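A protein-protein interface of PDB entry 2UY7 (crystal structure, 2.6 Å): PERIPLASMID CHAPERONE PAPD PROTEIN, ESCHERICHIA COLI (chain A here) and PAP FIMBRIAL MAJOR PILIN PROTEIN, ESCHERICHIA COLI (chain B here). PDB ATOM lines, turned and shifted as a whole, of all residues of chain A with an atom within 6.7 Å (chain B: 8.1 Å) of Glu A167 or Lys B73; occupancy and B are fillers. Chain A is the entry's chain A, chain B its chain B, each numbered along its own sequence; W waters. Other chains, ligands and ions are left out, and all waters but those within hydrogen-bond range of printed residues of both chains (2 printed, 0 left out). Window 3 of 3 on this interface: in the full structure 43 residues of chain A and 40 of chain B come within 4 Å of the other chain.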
ATOM      1  N   ILE A 154       0.824 -13.595   7.366  1.00  0.00           N
ATOM      2  CA  ILE A 154       0.611 -12.249   6.846  1.00  0.00           C
ATOM      3  C   ILE A 154      -0.372 -11.412   7.655  1.00  0.00           C
ATOM      4  O   ILE A 154      -0.658 -10.274   7.293  1.00  0.00           O
ATOM      5  CB  ILE A 154       0.087 -12.297   5.404  1.00  0.00           C
ATOM      6  CG1 ILE A 154      -1.278 -12.996   5.380  1.00  0.00           C
ATOM      7  CG2 ILE A 154       1.067 -13.047   4.526  1.00  0.00           C
ATOM      8  CD1 ILE A 154      -2.018 -12.867   4.061  1.00  0.00           C
ATOM      9  N   GLY A 155      -0.901 -11.973   8.737  1.00  0.00           N
ATOM     10  CA  GLY A 155      -1.836 -11.222   9.546  1.00  0.00           C
ATOM     11  C   GLY A 155      -2.158 -11.859  10.881  1.00  0.00           C
ATOM     12  O   GLY A 155      -2.208 -13.085  11.010  1.00  0.00           O
ATOM     13  N   LEU A 156      -2.358 -11.008  11.884  1.00  0.00           N
ATOM     14  CA  LEU A 156      -2.710 -11.440  13.236  1.00  0.00           C
ATOM     15  C   LEU A 156      -3.563 -10.331  13.838  1.00  0.00           C
ATOM     16  O   LEU A 156      -3.122  -9.193  13.933  1.00  0.00           O
ATOM     17  CB  LEU A 156      -1.458 -11.663  14.090  1.00  0.00           C
ATOM     18  CG  LEU A 156      -1.769 -12.138  15.518  1.00  0.00           C
ATOM     19  CD1 LEU A 156      -2.477 -13.482  15.466  1.00  0.00           C
ATOM     20  CD2 LEU A 156      -0.489 -12.251  16.328  1.00  0.00           C
ATOM     21  N   GLN A 162      -9.572  -7.933  10.753  1.00  0.00           N
ATOM     22  CA  GLN A 162      -8.307  -7.304  11.138  1.00  0.00           C
ATOM     23  C   GLN A 162      -7.105  -8.147  10.700  1.00  0.00           C
ATOM     24  O   GLN A 162      -6.070  -7.613  10.291  1.00  0.00           O
ATOM     25  CB  GLN A 162      -8.275  -7.094  12.652  1.00  0.00           C
ATOM     26  CG  GLN A 162      -7.108  -6.253  13.140  1.00  0.00           C
ATOM     27  CD  GLN A 162      -7.000  -6.236  14.653  1.00  0.00           C
ATOM     28  OE1 GLN A 162      -6.177  -5.520  15.215  1.00  0.00           O
ATOM     29  NE2 GLN A 162      -7.833  -7.032  15.322  1.00  0.00           N
ATOM     30  N   GLU A 165      -6.958  -7.339   6.801  1.00  0.00           N
ATOM     31  CA  GLU A 165      -6.552  -6.006   6.356  1.00  0.00           C
ATOM     32  C   GLU A 165      -5.685  -5.173   7.303  1.00  0.00           C
ATOM     33  O   GLU A 165      -5.252  -4.079   6.935  1.00  0.00           O
ATOM     34  CB  GLU A 165      -7.796  -5.209   5.956  1.00  0.00           C
ATOM     35  N   GLY A 166      -5.413  -5.681   8.502  1.00  0.00           N
ATOM     36  CA  GLY A 166      -4.615  -4.921   9.452  1.00  0.00           C
ATOM     37  C   GLY A 166      -3.121  -4.871   9.190  1.00  0.00           C
ATOM     38  O   GLY A 166      -2.543  -5.818   8.663  1.00  0.00           O
ATOM     39  N   GLU A 167      -2.493  -3.758   9.554  1.00  0.00           N
ATOM     40  CA  GLU A 167      -1.053  -3.600   9.385  1.00  0.00           C
ATOM     41  C   GLU A 167      -0.364  -4.793  10.019  1.00  0.00           C
ATOM     42  O   GLU A 167      -0.689  -5.186  11.140  1.00  0.00           O
ATOM     43  CB  GLU A 167      -0.570  -2.326  10.078  1.00  0.00           C
ATOM     44  CG  GLU A 167      -0.540  -1.103   9.190  1.00  0.00           C
ATOM     45  CD  GLU A 167       0.554  -1.183   8.144  1.00  0.00           C
ATOM     46  OE1 GLU A 167       0.632  -0.275   7.287  1.00  0.00           O
ATOM     47  OE2 GLU A 167       1.340  -2.158   8.182  1.00  0.00           O
ATOM     48  N   PHE A 168       0.589  -5.374   9.308  1.00  0.00           N
ATOM     49  CA  PHE A 168       1.304  -6.524   9.833  1.00  0.00           C
ATOM     50  C   PHE A 168       2.535  -6.767   8.992  1.00  0.00           C
ATOM     51  O   PHE A 168       2.471  -6.718   7.773  1.00  0.00           O
ATOM     52  CB  PHE A 168       0.416  -7.763   9.789  1.00  0.00           C
ATOM     53  CG  PHE A 168       1.003  -8.952  10.481  1.00  0.00           C
ATOM     54  CD1 PHE A 168       0.856  -9.117  11.855  1.00  0.00           C
ATOM     55  CD2 PHE A 168       1.726  -9.904   9.767  1.00  0.00           C
ATOM     56  CE1 PHE A 168       1.423 -10.214  12.512  1.00  0.00           C
ATOM     57  CE2 PHE A 168       2.295 -11.003  10.414  1.00  0.00           C
ATOM     58  CZ  PHE A 168       2.145 -11.159  11.785  1.00  0.00           C
ATOM     59  N   GLU A 169       3.662  -7.020   9.640  1.00  0.00           N
ATOM     60  CA  GLU A 169       4.894  -7.299   8.916  1.00  0.00           C
ATOM     61  C   GLU A 169       4.974  -8.805   8.653  1.00  0.00           C
ATOM     62  O   GLU A 169       5.183  -9.599   9.572  1.00  0.00           O
ATOM     63  CB  GLU A 169       6.097  -6.851   9.739  1.00  0.00           C
ATOM     64  CG  GLU A 169       7.427  -7.158   9.097  1.00  0.00           C
ATOM     65  CD  GLU A 169       8.577  -6.573   9.888  1.00  0.00           C
ATOM     66  OE1 GLU A 169       8.587  -5.334  10.079  1.00  0.00           O
ATOM     67  OE2 GLU A 169       9.466  -7.347  10.321  1.00  0.00           O
ATOM     68  N   THR B  64      -3.788  -5.346  -4.834  1.00  0.00           N
ATOM     69  CA  THR B  64      -4.064  -5.121  -3.417  1.00  0.00           C
ATOM     70  C   THR B  64      -2.860  -5.568  -2.587  1.00  0.00           C
ATOM     71  O   THR B  64      -3.008  -6.301  -1.607  1.00  0.00           O
ATOM     72  CB  THR B  64      -5.321  -5.892  -2.991  1.00  0.00           C
ATOM     73  N   ALA B  65      -1.672  -5.122  -2.997  1.00  0.00           N
ATOM     74  CA  ALA B  65      -0.414  -5.449  -2.325  1.00  0.00           C
ATOM     75  C   ALA B  65       0.640  -4.375  -2.606  1.00  0.00           C
ATOM     76  O   ALA B  65       1.659  -4.297  -1.926  1.00  0.00           O
ATOM     77  CB  ALA B  65       0.089  -6.813  -2.786  1.00  0.00           C
ATOM     78  N   LYS B  67       0.798  -0.887  -2.204  1.00  0.00           N
ATOM     79  CA  LYS B  67       0.176   0.298  -1.616  1.00  0.00           C
ATOM     80  C   LYS B  67      -1.316  -0.016  -1.634  1.00  0.00           C
ATOM     81  O   LYS B  67      -2.157   0.844  -1.387  1.00  0.00           O
ATOM     82  CB  LYS B  67       0.477   1.551  -2.453  1.00  0.00           C
ATOM     83  N   GLY B  68      -1.613  -1.275  -1.951  1.00  0.00           N
ATOM     84  CA  GLY B  68      -2.974  -1.771  -2.004  1.00  0.00           C
ATOM     85  C   GLY B  68      -3.979  -1.015  -2.849  1.00  0.00           C
ATOM     86  O   GLY B  68      -3.871   0.193  -3.060  1.00  0.00           O
ATOM     87  N   GLY B  69      -4.965  -1.751  -3.345  1.00  0.00           N
ATOM     88  CA  GLY B  69      -6.014  -1.149  -4.141  1.00  0.00           C
ATOM     89  C   GLY B  69      -7.199  -0.976  -3.212  1.00  0.00           C
ATOM     90  O   GLY B  69      -7.706  -1.956  -2.660  1.00  0.00           O
ATOM     91  N   ASN B  70      -7.637   0.267  -3.029  1.00  0.00           N
ATOM     92  CA  ASN B  70      -8.757   0.573  -2.144  1.00  0.00           C
ATOM     93  C   ASN B  70      -8.344   0.293  -0.698  1.00  0.00           C
ATOM     94  O   ASN B  70      -9.176  -0.070   0.140  1.00  0.00           O
ATOM     95  CB  ASN B  70      -9.989  -0.266  -2.523  1.00  0.00           C
ATOM     96  N   GLY B  71      -7.050   0.462  -0.420  1.00  0.00           N
ATOM     97  CA  GLY B  71      -6.528   0.235   0.919  1.00  0.00           C
ATOM     98  C   GLY B  71      -5.312  -0.679   0.992  1.00  0.00           C
ATOM     99  O   GLY B  71      -4.297  -0.432   0.338  1.00  0.00           O
ATOM    100  N   ALA B  72      -5.417  -1.736   1.798  1.00  0.00           N
ATOM    101  CA  ALA B  72      -4.336  -2.706   1.979  1.00  0.00           C
ATOM    102  C   ALA B  72      -3.084  -2.060   2.578  1.00  0.00           C
ATOM    103  O   ALA B  72      -2.370  -1.313   1.903  1.00  0.00           O
ATOM    104  CB  ALA B  72      -4.001  -3.371   0.647  1.00  0.00           C
ATOM    105  N   LYS B  73      -2.822  -2.359   3.847  1.00  0.00           N
ATOM    106  CA  LYS B  73      -1.664  -1.814   4.545  1.00  0.00           C
ATOM    107  C   LYS B  73      -0.509  -2.821   4.628  1.00  0.00           C
ATOM    108  O   LYS B  73       0.650  -2.435   4.794  1.00  0.00           O
ATOM    109  CB  LYS B  73      -2.077  -1.367   5.944  1.00  0.00           C
ATOM    110  N   LYS B  74      -0.826  -4.109   4.512  1.00  0.00           N
ATOM    111  CA  LYS B  74       0.189  -5.165   4.570  1.00  0.00           C
ATOM    112  C   LYS B  74       1.109  -5.114   3.344  1.00  0.00           C
ATOM    113  O   LYS B  74       0.835  -4.402   2.370  1.00  0.00           O
ATOM    114  CB  LYS B  74      -0.471  -6.547   4.619  1.00  0.00           C
ATOM    115  CG  LYS B  74      -1.547  -6.717   5.671  1.00  0.00           C
ATOM    116  CD  LYS B  74      -2.145  -8.113   5.583  1.00  0.00           C
ATOM    117  CE  LYS B  74      -3.250  -8.326   6.600  1.00  0.00           C
ATOM    118  NZ  LYS B  74      -2.804  -8.196   8.008  1.00  0.00           N
ATOM    119  N   GLY B  75       2.190  -5.890   3.400  1.00  0.00           N
ATOM    120  CA  GLY B  75       3.144  -5.944   2.304  1.00  0.00           C
ATOM    121  C   GLY B  75       3.513  -7.378   1.975  1.00  0.00           C
ATOM    122  O   GLY B  75       4.347  -7.991   2.636  1.00  0.00           O
ATOM    123  N   THR B  76       2.887  -7.917   0.938  1.00  0.00           N
ATOM    124  CA  THR B  76       3.138  -9.288   0.527  1.00  0.00           C
ATOM    125  C   THR B  76       4.143  -9.405  -0.629  1.00  0.00           C
ATOM    126  O   THR B  76       4.596 -10.500  -0.958  1.00  0.00           O
ATOM    127  CB  THR B  76       1.800  -9.953   0.162  1.00  0.00           C
ATOM    128  OG1 THR B  76       1.484 -10.929   1.160  1.00  0.00           O
ATOM    129  CG2 THR B  76       1.851 -10.597  -1.209  1.00  0.00           C
ATOM    130  N   ALA B 121       6.877   0.417  -2.290  1.00  0.00           N
ATOM    131  CA  ALA B 121       5.688  -0.165  -2.917  1.00  0.00           C
ATOM    132  C   ALA B 121       4.499   0.698  -2.505  1.00  0.00           C
ATOM    133  O   ALA B 121       3.515   0.203  -1.960  1.00  0.00           O
ATOM    134  CB  ALA B 121       5.491  -1.605  -2.439  1.00  0.00           C
HETATM  135  O   HOH W   1      -3.095  -8.559  10.859  1.00  0.00           O
HETATM  136  O   HOH W   2       3.315  -7.507   5.054  1.00  0.00           O
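The side-chain amino group of Lys B74 sits at hydrogen-bond distance from the backbone carbonyl oxygen of Gly A166 (2.5 Å).
The backbone carbonyl oxygen (O) of Lys B73 sits close to the side-chain carboxylate (OE1) of Glu A167, 3.3 Å away.
The side-chain amino group (NZ) of Lys B74 sits at hydrogen-bond distance from the backbone carbonyl oxygen (O) of Ile A154.
Among the printed residues, merely in contact across the chains: Ile A154 with Thr B76, Gly A155 with Lys B74, Glu A165 with Lys B74 and Phe A168 with Lys B74.
Water W2 lies within hydrogen-bond range of the backbone NH of Gly B75 and the backbone carbonyl oxygen of Phe A168.
Water W1 lies within hydrogen-bond range of the backbone NH (N) of Leu A156, the side-chain amino group (NZ) of Lys B74 and the backbone carbonyl oxygen (O) of Gln A162.
Of the 9 printed residues of chain A, 6 touch a printed residue of chain B.
Hydrophobic or aromatic side chains of chain A within 4 Å of the printed part of chain B: Ile A154 and Phe A168.
Among the printed residues, no Asp or Glu carboxylate lies within 4 Å of a Lys or Arg side-chain nitrogen of the other chain.
Printed residues of chain B within 4 Å of Ile A154: Lys B74 (3.1 Å) and Thr B76 (3.999 Å).
Of the printed residues of chain B, Gly A155 touches Lys B74 (3.5 Å).
Gly A166 touches just one residue of chain B: Lys B74.
Glu A167 touches just one residue of chain B: Lys B73 (3.2 Å).
Of the printed residues of chain B, Phe A168 touches Lys B74.
Of chain A, only Glu A167 (3.2 Å) comes within 4 Å of Lys B73.
Of the printed residues of chain A, Lys B74 touches Ile A154, Gly A155, Glu A165, Gly A166 and Phe A168.
The nearest residue of chain B that does not touch Glu A167 is Lys B74 (4.6 Å).
The nearest residue of chain A that does not touch Lys B73 is Glu A165 (4.3 Å).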
